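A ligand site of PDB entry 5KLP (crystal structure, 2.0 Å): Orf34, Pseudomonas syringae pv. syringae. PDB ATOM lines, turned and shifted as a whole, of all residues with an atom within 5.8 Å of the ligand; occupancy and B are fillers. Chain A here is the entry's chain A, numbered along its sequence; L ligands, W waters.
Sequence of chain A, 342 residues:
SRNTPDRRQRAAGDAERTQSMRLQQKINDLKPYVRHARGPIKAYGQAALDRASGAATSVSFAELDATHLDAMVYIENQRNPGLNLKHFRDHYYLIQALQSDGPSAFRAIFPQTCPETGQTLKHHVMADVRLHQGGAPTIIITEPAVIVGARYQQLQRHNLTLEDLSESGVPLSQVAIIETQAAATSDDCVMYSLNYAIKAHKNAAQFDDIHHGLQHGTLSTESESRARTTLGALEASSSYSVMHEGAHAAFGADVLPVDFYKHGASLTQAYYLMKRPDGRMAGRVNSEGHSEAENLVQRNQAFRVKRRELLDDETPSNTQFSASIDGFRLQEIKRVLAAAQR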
ATOM      1  N   ARG A  22      32.255  14.900  16.852  1.00  0.00           N
ATOM      2  CA  ARG A  22      30.833  15.142  17.105  1.00  0.00           C
ATOM      3  C   ARG A  22      30.353  16.419  16.438  1.00  0.00           C
ATOM      4  O   ARG A  22      29.257  16.463  15.860  1.00  0.00           O
ATOM      5  CB  ARG A  22      30.548  15.213  18.598  1.00  0.00           C
ATOM      6  CG  ARG A  22      30.642  13.880  19.327  1.00  0.00           C
ATOM      7  CD  ARG A  22      29.352  13.095  19.135  1.00  0.00           C
ATOM      8  NE  ARG A  22      28.308  13.544  20.057  1.00  0.00           N
ATOM      9  CZ  ARG A  22      28.308  13.368  21.368  1.00  0.00           C
ATOM     10  NH1 ARG A  22      29.313  12.730  21.967  1.00  0.00           N
ATOM     11  NH2 ARG A  22      27.300  13.828  22.101  1.00  0.00           N
ATOM     12  N   LYS A  26      27.824  17.241  12.951  1.00  0.00           N
ATOM     13  CA  LYS A  26      26.753  18.231  12.892  1.00  0.00           C
ATOM     14  C   LYS A  26      26.987  19.203  11.739  1.00  0.00           C
ATOM     15  O   LYS A  26      26.044  19.640  11.095  1.00  0.00           O
ATOM     16  CB  LYS A  26      26.598  18.977  14.213  1.00  0.00           C
ATOM     17  CG  LYS A  26      26.074  18.098  15.341  1.00  0.00           C
ATOM     18  CD  LYS A  26      25.913  18.918  16.607  1.00  0.00           C
ATOM     19  CE  LYS A  26      25.320  18.105  17.759  1.00  0.00           C
ATOM     20  NZ  LYS A  26      23.833  18.120  17.794  1.00  0.00           N
ATOM     21  N   GLU A  76      10.267  25.033  16.362  1.00  0.00           N
ATOM     22  CA  GLU A  76      10.311  24.247  17.588  1.00  0.00           C
ATOM     23  C   GLU A  76       8.929  24.130  18.223  1.00  0.00           C
ATOM     24  O   GLU A  76       8.587  23.095  18.793  1.00  0.00           O
ATOM     25  CB  GLU A  76      11.312  24.855  18.564  1.00  0.00           C
ATOM     26  CG  GLU A  76      12.793  24.657  18.220  1.00  0.00           C
ATOM     27  CD  GLU A  76      13.219  23.176  18.149  1.00  0.00           C
ATOM     28  OE1 GLU A  76      12.441  22.288  18.547  1.00  0.00           O
ATOM     29  OE2 GLU A  76      14.368  22.900  17.730  1.00  0.00           O
ATOM     30  N   ARG A  79       7.509  21.259  16.328  1.00  0.00           N
ATOM     31  CA  ARG A  79       8.128  19.964  16.653  1.00  0.00           C
ATOM     32  C   ARG A  79       7.630  19.456  18.002  1.00  0.00           C
ATOM     33  O   ARG A  79       7.472  18.249  18.192  1.00  0.00           O
ATOM     34  CB  ARG A  79       9.662  20.071  16.698  1.00  0.00           C
ATOM     35  CG  ARG A  79      10.313  20.455  15.362  1.00  0.00           C
ATOM     36  CD  ARG A  79      11.845  20.415  15.384  1.00  0.00           C
ATOM     37  NE  ARG A  79      12.389  19.117  15.782  1.00  0.00           N
ATOM     38  CZ  ARG A  79      12.797  18.786  17.006  1.00  0.00           C
ATOM     39  NH1 ARG A  79      12.749  19.662  18.009  1.00  0.00           N
ATOM     40  NH2 ARG A  79      13.266  17.563  17.219  1.00  0.00           N
ATOM     41  N   ASN A  80       7.406  20.377  18.937  1.00  0.00           N
ATOM     42  CA  ASN A  80       7.013  20.030  20.306  1.00  0.00           C
ATOM     43  C   ASN A  80       5.798  20.826  20.741  1.00  0.00           C
ATOM     44  O   ASN A  80       5.943  21.806  21.470  1.00  0.00           O
ATOM     45  CB  ASN A  80       8.150  20.304  21.291  1.00  0.00           C
ATOM     46  CG  ASN A  80       9.477  19.784  20.816  1.00  0.00           C
ATOM     47  OD1 ASN A  80       9.758  18.595  20.909  1.00  0.00           O
ATOM     48  ND2 ASN A  80      10.326  20.683  20.295  1.00  0.00           N
ATOM     49  N   ASN A 195      17.789  26.872  23.724  1.00  0.00           N
ATOM     50  CA  ASN A 195      17.974  25.533  24.244  1.00  0.00           C
ATOM     51  C   ASN A 195      17.291  25.377  25.591  1.00  0.00           C
ATOM     52  O   ASN A 195      16.656  24.353  25.862  1.00  0.00           O
ATOM     53  CB  ASN A 195      19.459  25.181  24.395  1.00  0.00           C
ATOM     54  CG  ASN A 195      19.676  23.742  24.851  1.00  0.00           C
ATOM     55  OD1 ASN A 195      19.780  23.478  26.037  1.00  0.00           O
ATOM     56  ND2 ASN A 195      19.700  22.814  23.895  1.00  0.00           N
ATOM     57  N   ILE A 198      13.497  24.843  25.359  1.00  0.00           N
ATOM     58  CA  ILE A 198      13.219  23.441  25.024  1.00  0.00           C
ATOM     59  C   ILE A 198      13.410  22.535  26.244  1.00  0.00           C
ATOM     60  O   ILE A 198      12.599  21.635  26.499  1.00  0.00           O
ATOM     61  CB  ILE A 198      14.115  22.928  23.872  1.00  0.00           C
ATOM     62  CG1 ILE A 198      13.894  23.786  22.617  1.00  0.00           C
ATOM     63  CG2 ILE A 198      13.815  21.453  23.579  1.00  0.00           C
ATOM     64  CD1 ILE A 198      14.869  23.489  21.484  1.00  0.00           C
ATOM     65  N   LYS A 199      14.490  22.754  26.998  1.00  0.00           N
ATOM     66  CA  LYS A 199      14.741  21.925  28.188  1.00  0.00           C
ATOM     67  C   LYS A 199      13.694  22.160  29.272  1.00  0.00           C
ATOM     68  O   LYS A 199      13.324  21.232  30.004  1.00  0.00           O
ATOM     69  CB  LYS A 199      16.149  22.183  28.763  1.00  0.00           C
ATOM     70  CG  LYS A 199      17.290  21.819  27.814  1.00  0.00           C
ATOM     71  CD  LYS A 199      17.112  20.411  27.236  1.00  0.00           C
ATOM     72  CE  LYS A 199      18.318  19.993  26.425  1.00  0.00           C
ATOM     73  NZ  LYS A 199      18.104  18.670  25.793  1.00  0.00           N
ATOM     74  N   LYS A 202      10.835  20.116  28.213  1.00  0.00           N
ATOM     75  CA  LYS A 202      11.077  18.698  28.443  1.00  0.00           C
ATOM     76  C   LYS A 202      11.011  18.341  29.921  1.00  0.00           C
ATOM     77  O   LYS A 202      10.625  17.232  30.283  1.00  0.00           O
ATOM     78  CB  LYS A 202      12.436  18.263  27.884  1.00  0.00           C
ATOM     79  CG  LYS A 202      12.519  18.131  26.380  1.00  0.00           C
ATOM     80  CD  LYS A 202      13.846  17.504  25.975  1.00  0.00           C
ATOM     81  CE  LYS A 202      13.832  17.048  24.505  1.00  0.00           C
ATOM     82  NZ  LYS A 202      14.541  17.937  23.573  1.00  0.00           N
ATOM     83  N   LYS A 262      24.530  20.863  29.623  1.00  0.00           N
ATOM     84  CA  LYS A 262      25.069  20.116  28.504  1.00  0.00           C
ATOM     85  C   LYS A 262      25.886  20.962  27.510  1.00  0.00           C
ATOM     86  O   LYS A 262      26.807  20.448  26.863  1.00  0.00           O
ATOM     87  CB  LYS A 262      23.915  19.420  27.741  1.00  0.00           C
ATOM     88  CG  LYS A 262      23.315  18.246  28.468  1.00  0.00           C
ATOM     89  CD  LYS A 262      22.284  17.527  27.602  1.00  0.00           C
ATOM     90  CE  LYS A 262      22.958  16.717  26.483  1.00  0.00           C
ATOM     91  NZ  LYS A 262      21.962  15.884  25.728  1.00  0.00           N
ATOM     92  N   HIS A 263      25.551  22.243  27.369  1.00  0.00           N
ATOM     93  CA  HIS A 263      26.265  23.120  26.432  1.00  0.00           C
ATOM     94  C   HIS A 263      27.223  24.074  27.120  1.00  0.00           C
ATOM     95  O   HIS A 263      27.677  25.050  26.515  1.00  0.00           O
ATOM     96  CB  HIS A 263      25.258  23.890  25.578  1.00  0.00           C
ATOM     97  CG  HIS A 263      24.370  22.988  24.787  1.00  0.00           C
ATOM     98  ND1 HIS A 263      24.851  22.183  23.777  1.00  0.00           N
ATOM     99  CD2 HIS A 263      23.047  22.713  24.898  1.00  0.00           C
ATOM    100  CE1 HIS A 263      23.863  21.463  23.282  1.00  0.00           C
ATOM    101  NE2 HIS A 263      22.754  21.767  23.942  1.00  0.00           N
ATOM    102  N   VAL A 285      23.818  12.109  30.375  1.00  0.00           N
ATOM    103  CA  VAL A 285      23.216  13.304  29.787  1.00  0.00           C
ATOM    104  C   VAL A 285      22.720  13.092  28.361  1.00  0.00           C
ATOM    105  O   VAL A 285      22.020  13.940  27.823  1.00  0.00           O
ATOM    106  CB  VAL A 285      24.194  14.501  29.813  1.00  0.00           C
ATOM    107  CG1 VAL A 285      24.551  14.883  31.255  1.00  0.00           C
ATOM    108  CG2 VAL A 285      25.454  14.214  28.998  1.00  0.00           C
ATOM    109  N   ASN A 286      23.034  11.952  27.753  1.00  0.00           N
ATOM    110  CA  ASN A 286      22.469  11.644  26.440  1.00  0.00           C
ATOM    111  C   ASN A 286      21.321  10.654  26.554  1.00  0.00           C
ATOM    112  O   ASN A 286      21.211   9.959  27.547  1.00  0.00           O
ATOM    113  CB  ASN A 286      23.541  11.100  25.498  1.00  0.00           C
ATOM    114  CG  ASN A 286      24.060   9.733  25.919  1.00  0.00           C
ATOM    115  OD1 ASN A 286      23.986   9.357  27.085  1.00  0.00           O
ATOM    116  ND2 ASN A 286      24.561   8.981  24.947  1.00  0.00           N
ATOM    117  N   SER A 287      20.469  10.579  25.526  1.00  0.00           N
ATOM    118  CA  SER A 287      19.293   9.721  25.627  1.00  0.00           C
ATOM    119  C   SER A 287      19.698   8.246  25.648  1.00  0.00           C
ATOM    120  O   SER A 287      20.789   7.880  25.181  1.00  0.00           O
ATOM    121  CB  SER A 287      18.326   9.978  24.466  1.00  0.00           C
ATOM    122  OG  SER A 287      18.915   9.605  23.231  1.00  0.00           O
ATOM    123  N   HIS A 290      21.092   5.725  22.764  1.00  0.00           N
ATOM    124  CA  HIS A 290      22.507   5.603  22.446  1.00  0.00           C
ATOM    125  C   HIS A 290      23.072   4.368  23.121  1.00  0.00           C
ATOM    126  O   HIS A 290      22.705   4.042  24.264  1.00  0.00           O
ATOM    127  CB  HIS A 290      23.278   6.848  22.872  1.00  0.00           C
ATOM    128  CG  HIS A 290      23.082   8.025  21.975  1.00  0.00           C
ATOM    129  ND1 HIS A 290      23.791   8.202  20.807  1.00  0.00           N
ATOM    130  CD2 HIS A 290      22.259   9.094  22.068  1.00  0.00           C
ATOM    131  CE1 HIS A 290      23.408   9.324  20.215  1.00  0.00           C
ATOM    132  NE2 HIS A 290      22.474   9.882  20.972  1.00  0.00           N
ATOM    133  N   GLU A 294      26.913   8.775  28.206  1.00  0.00           N
ATOM    134  CA  GLU A 294      27.797   9.920  28.172  1.00  0.00           C
ATOM    135  C   GLU A 294      27.441  10.827  29.343  1.00  0.00           C
ATOM    136  O   GLU A 294      26.273  11.150  29.544  1.00  0.00           O
ATOM    137  CB  GLU A 294      27.667  10.646  26.827  1.00  0.00           C
ATOM    138  CG  GLU A 294      28.503  11.900  26.683  1.00  0.00           C
ATOM    139  CD  GLU A 294      28.509  12.424  25.252  1.00  0.00           C
ATOM    140  OE1 GLU A 294      27.434  12.778  24.720  1.00  0.00           O
ATOM    141  OE2 GLU A 294      29.603  12.494  24.665  1.00  0.00           O
ATOM    142  N   ARG A 299      30.875  14.586  27.554  1.00  0.00           N
ATOM    143  CA  ARG A 299      30.259  15.394  26.513  1.00  0.00           C
ATOM    144  C   ARG A 299      31.118  16.616  26.217  1.00  0.00           C
ATOM    145  O   ARG A 299      31.429  16.902  25.048  1.00  0.00           O
ATOM    146  CB  ARG A 299      28.846  15.839  26.909  1.00  0.00           C
ATOM    147  CG  ARG A 299      28.249  16.709  25.835  1.00  0.00           C
ATOM    148  CD  ARG A 299      26.858  17.243  26.150  1.00  0.00           C
ATOM    149  NE  ARG A 299      26.479  18.090  25.021  1.00  0.00           N
ATOM    150  CZ  ARG A 299      25.889  17.656  23.908  1.00  0.00           C
ATOM    151  NH1 ARG A 299      25.558  16.375  23.777  1.00  0.00           N
ATOM    152  NH2 ARG A 299      25.621  18.505  22.930  1.00  0.00           N
ATOM    153  N   PHE A 303      33.192  17.694  22.551  1.00  0.00           N
ATOM    154  CA  PHE A 303      32.994  18.926  21.816  1.00  0.00           C
ATOM    155  C   PHE A 303      34.131  19.930  22.029  1.00  0.00           C
ATOM    156  O   PHE A 303      33.996  21.110  21.669  1.00  0.00           O
ATOM    157  CB  PHE A 303      31.657  19.570  22.206  1.00  0.00           C
ATOM    158  CG  PHE A 303      30.461  18.867  21.614  1.00  0.00           C
ATOM    159  CD1 PHE A 303      29.998  19.203  20.353  1.00  0.00           C
ATOM    160  CD2 PHE A 303      29.847  17.834  22.293  1.00  0.00           C
ATOM    161  CE1 PHE A 303      28.907  18.553  19.786  1.00  0.00           C
ATOM    162  CE2 PHE A 303      28.746  17.164  21.746  1.00  0.00           C
ATOM    163  CZ  PHE A 303      28.273  17.536  20.486  1.00  0.00           C
ATOM    164  N   SER A 324      30.032  22.871  22.113  1.00  0.00           N
ATOM    165  CA  SER A 324      28.721  22.223  22.077  1.00  0.00           C
ATOM    166  C   SER A 324      27.562  23.153  21.676  1.00  0.00           C
ATOM    167  O   SER A 324      26.667  22.743  20.932  1.00  0.00           O
ATOM    168  CB  SER A 324      28.429  21.580  23.443  1.00  0.00           C
ATOM    169  OG  SER A 324      27.173  20.916  23.452  1.00  0.00           O
ATOM    170  N   PHE A 328      24.623  23.025  18.799  1.00  0.00           N
ATOM    171  CA  PHE A 328      23.183  23.210  18.958  1.00  0.00           C
ATOM    172  C   PHE A 328      22.653  24.184  17.881  1.00  0.00           C
ATOM    173  O   PHE A 328      21.576  23.959  17.327  1.00  0.00           O
ATOM    174  CB  PHE A 328      22.851  23.731  20.370  1.00  0.00           C
ATOM    175  CG  PHE A 328      21.391  24.060  20.558  1.00  0.00           C
ATOM    176  CD1 PHE A 328      20.437  23.059  20.605  1.00  0.00           C
ATOM    177  CD2 PHE A 328      20.983  25.382  20.640  1.00  0.00           C
ATOM    178  CE1 PHE A 328      19.088  23.362  20.756  1.00  0.00           C
ATOM    179  CE2 PHE A 328      19.635  25.696  20.782  1.00  0.00           C
ATOM    180  CZ  PHE A 328      18.689  24.681  20.833  1.00  0.00           C
ATOM    181  N   GLN A 331      22.208  22.386  14.694  1.00  0.00           N
ATOM    182  CA  GLN A 331      21.026  21.549  14.821  1.00  0.00           C
ATOM    183  C   GLN A 331      19.735  22.325  14.569  1.00  0.00           C
ATOM    184  O   GLN A 331      18.826  21.849  13.877  1.00  0.00           O
ATOM    185  CB  GLN A 331      20.985  20.924  16.217  1.00  0.00           C
ATOM    186  CG  GLN A 331      19.648  20.329  16.585  1.00  0.00           C
ATOM    187  CD  GLN A 331      19.613  19.888  18.045  1.00  0.00           C
ATOM    188  OE1 GLN A 331      20.190  18.863  18.404  1.00  0.00           O
ATOM    189  NE2 GLN A 331      18.970  20.690  18.887  1.00  0.00           N
ATOM    190  N   GLU A 332      19.661  23.543  15.118  1.00  0.00           N
ATOM    191  CA  GLU A 332      18.457  24.357  14.979  1.00  0.00           C
ATOM    192  C   GLU A 332      18.256  24.844  13.533  1.00  0.00           C
ATOM    193  O   GLU A 332      17.149  24.840  13.030  1.00  0.00           O
ATOM    194  CB  GLU A 332      18.527  25.542  15.928  1.00  0.00           C
ATOM    195  CG  GLU A 332      18.483  25.095  17.367  1.00  0.00           C
ATOM    196  CD  GLU A 332      17.342  24.138  17.625  1.00  0.00           C
ATOM    197  OE1 GLU A 332      16.199  24.625  17.742  1.00  0.00           O
ATOM    198  OE2 GLU A 332      17.585  22.904  17.686  1.00  0.00           O
ATOM    199  N   ARG A 335      17.023  22.033  11.547  1.00  0.00           N
ATOM    200  CA  ARG A 335      15.593  21.818  11.766  1.00  0.00           C
ATOM    201  C   ARG A 335      14.745  22.811  10.963  1.00  0.00           C
ATOM    202  O   ARG A 335      13.720  22.448  10.405  1.00  0.00           O
ATOM    203  CB  ARG A 335      15.277  21.881  13.244  1.00  0.00           C
ATOM    204  CG  ARG A 335      15.698  20.616  13.983  1.00  0.00           C
ATOM    205  CD  ARG A 335      15.587  20.779  15.503  1.00  0.00           C
ATOM    206  NE  ARG A 335      16.060  19.580  16.169  1.00  0.00           N
ATOM    207  CZ  ARG A 335      16.150  19.433  17.484  1.00  0.00           C
ATOM    208  NH1 ARG A 335      15.765  20.424  18.278  1.00  0.00           N
ATOM    209  NH2 ARG A 335      16.604  18.305  18.002  1.00  0.00           N
HETATM  210  C1  LIG L   1      17.770  16.126  20.050  1.00  0.00           C
HETATM  211  C2  LIG L   1      18.515  17.274  20.865  1.00  0.00           C
HETATM  212  C3  LIG L   1      20.073  17.270  21.111  1.00  0.00           C
HETATM  213  C4  LIG L   1      20.811  15.972  20.560  1.00  0.00           C
HETATM  214  C5  LIG L   1      19.986  14.721  20.329  1.00  0.00           C
HETATM  215  C6  LIG L   1      18.845  15.163  19.411  1.00  0.00           C
HETATM  216  O1  LIG L   1      16.858  15.507  20.752  1.00  0.00           O
HETATM  217  P1  LIG L   1      15.192  15.327  20.502  1.00  0.00           P
HETATM  218  O2  LIG L   1      14.445  15.435  21.824  1.00  0.00           O
HETATM  219  O3  LIG L   1      14.913  13.938  19.904  1.00  0.00           O
HETATM  220  O4  LIG L   1      14.580  16.347  19.555  1.00  0.00           O
HETATM  221  O5  LIG L   1      17.849  17.634  22.022  1.00  0.00           O
HETATM  222  P2  LIG L   1      17.244  19.204  22.101  1.00  0.00           P
HETATM  223  O6  LIG L   1      16.239  19.430  20.954  1.00  0.00           O
HETATM  224  O7  LIG L   1      16.569  19.554  23.429  1.00  0.00           O
HETATM  225  O8  LIG L   1      18.400  20.190  21.824  1.00  0.00           O
HETATM  226  O9  LIG L   1      20.224  17.400  22.369  1.00  0.00           O
HETATM  227  P3  LIG L   1      20.941  18.530  23.401  1.00  0.00           P
HETATM  228  O10 LIG L   1      20.418  19.965  23.370  1.00  0.00           O
HETATM  229  O11 LIG L   1      20.440  17.840  24.664  1.00  0.00           O
HETATM  230  O12 LIG L   1      22.463  18.548  23.342  1.00  0.00           O
HETATM  231  O13 LIG L   1      21.898  15.661  21.301  1.00  0.00           O
HETATM  232  P4  LIG L   1      23.405  16.090  20.877  1.00  0.00           P
HETATM  233  O14 LIG L   1      23.684  17.556  21.217  1.00  0.00           O
HETATM  234  O15 LIG L   1      24.464  15.193  21.559  1.00  0.00           O
HETATM  235  O16 LIG L   1      23.607  15.924  19.363  1.00  0.00           O
HETATM  236  O17 LIG L   1      19.649  14.014  21.414  1.00  0.00           O
HETATM  237  P5  LIG L   1      20.258  12.452  21.742  1.00  0.00           P
HETATM  238  O18 LIG L   1      21.449  12.129  20.830  1.00  0.00           O
HETATM  239  O19 LIG L   1      20.754  12.356  23.211  1.00  0.00           O
HETATM  240  O20 LIG L   1      19.212  11.360  21.525  1.00  0.00           O
HETATM  241  O21 LIG L   1      18.268  14.110  18.849  1.00  0.00           O
HETATM  242  P6  LIG L   1      17.657  14.085  17.329  1.00  0.00           P
HETATM  243  O22 LIG L   1      18.532  14.912  16.390  1.00  0.00           O
HETATM  244  O23 LIG L   1      17.570  12.648  16.783  1.00  0.00           O
HETATM  245  O24 LIG L   1      16.233  14.656  17.300  1.00  0.00           O
HETATM  246  O   HOH W   1      19.457  14.339  24.850  1.00  0.00           O
HETATM  247  O   HOH W   2      24.141  12.503  21.214  1.00  0.00           O
HETATM  248  O   HOH W   3      16.601  12.464  21.880  1.00  0.00           O
HETATM  249  O   HOH W   4      22.789  19.644  19.636  1.00  0.00           O
HETATM  250  O   HOH W   5      25.538  20.135  20.192  1.00  0.00           O
HETATM  251  O   HOH W   6      13.653  18.844  20.725  1.00  0.00           O
HETATM  252  O   HOH W   7      21.087  16.973  16.493  1.00  0.00           O
HETATM  253  O   HOH W   8      22.724  14.171  17.333  1.00  0.00           O
HETATM  254  O   HOH W   9      26.055  14.814  18.871  1.00  0.00           O
HETATM  255  O   HOH W  10      22.830  13.970  23.916  1.00  0.00           O
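N of Ser 287 sits at hydrogen-bond distance from O19 of the ligand (2.9 Å).
O20 of the ligand is in hydrogen-bond range of OG of Ser 287.
A ring nitrogen (NE2) of His 290 sits at hydrogen-bond distance from an oxygen (O18) of the ligand (2.5 Å).
O7 of the ligand is in salt-bridge range of NZ of Lys 202 (2.6 Å).
NZ of Lys 262 lies within salt-bridge range of O11 of the ligand, at 2.7 Å.
The side-chain amino group of Lys 26 is in salt-bridge range of an oxygen (O16) of the ligand (2.7 Å).
O11 of the ligand is in salt-bridge range of NZ of Lys 199.
O15 of the ligand is in salt-bridge range of NH1 of Arg 299, at 2.7 Å.
NH1 of Arg 335 is in salt-bridge range of O6 of the ligand (2.9 Å).
An oxygen (O4) of the ligand is in salt-bridge range of the guanidinium group of Arg 79.
The side-chain amide nitrogen (ND2) of Asn 195 is in hydrogen-bond range of an oxygen (O10) of the ligand (3.0 Å).
NE2 of His 263 lies within hydrogen-bond range of O10 of the ligand (3.0 Å).
NE2 of Gln 331 is in hydrogen-bond range of O8 of the ligand (3.0 Å).
The guanidinium group (NH2) of Arg 22 is in salt-bridge range of an oxygen (O15) of the ligand (3.2 Å).
The backbone carbonyl oxygen (O) of Lys 262 lies within hydrogen-bond range of the guanidinium group (NE) of Arg 299 (3.0 Å).
The side-chain amino group (NZ) of Lys 262 sits at hydrogen-bond distance from the backbone carbonyl oxygen (O) of Val 285, 2.9 Å away.
The side-chain hydroxyl of Ser 324 is in hydrogen-bond range of the backbone carbonyl oxygen of Lys 262, at 3.5 Å.
The guanidinium group of Arg 299 lies within hydrogen-bond range of the side-chain hydroxyl of Ser 324 (2.9 Å).
The guanidinium group (NH1) of Arg 335 lies within salt-bridge range of the side-chain carboxylate (OE2) of Glu 332 (3.1 Å).
NH1 of Arg 79 lies within salt-bridge range of OE1 of Glu 76.
The side-chain carboxylate of Glu 294 lies within salt-bridge range of the guanidinium group of Arg 22 (2.7 Å).
The backbone NH (N) of Glu 294 is in hydrogen-bond range of the side-chain amide oxygen (OD1) of Asn 286, 3.2 Å away.
Ile 198 touches the ligand.
Asn 286 touches the ligand (CA to O19, 3.7 Å).
Phe 328 touches the ligand (CE1 to O8, 3.4 Å).
Hydrophobic or aromatic side chains that line the ligand: Ile 198, His 263, His 290 and Phe 328.
Within 4 Å of the ligand: Arg 22, Lys 26, Arg 79, Asn 195, Ile 198, Lys 199, Lys 202, Lys 262, His 263, Asn 286, Ser 287, His 290, Arg 299, Phe 328, Gln 331 and Arg 335.
The nearest printed residue that does not touch the ligand is Phe 303 (4.6 Å).
Water W6 lies within hydrogen-bond range of an oxygen (O6) of the ligand, the guanidinium group (NH1) of Arg 79 and the side-chain amino group (NZ) of Lys 202.
Water W10 bridges an oxygen (O19) of the ligand and the side-chain amino group of Lys 262.
Water W2 bridges O15 of the ligand and NE2 of His 290.
Water W9 bridges an oxygen (O16) of the ligand (2.7 Å) and the guanidinium group of Arg 22 (2.8 Å).
Water W4 lies within hydrogen-bond range of NZ of Lys 26, O14 of the ligand and OE1 of Gln 331.
Water W5 lies within hydrogen-bond range of the backbone carbonyl oxygen of Ser 324 (2.9 Å), the guanidinium group of Arg 299 (3.2 Å), the backbone NH of Phe 328 (3.3 Å) and an oxygen (O14) of the ligand (3.3 Å).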
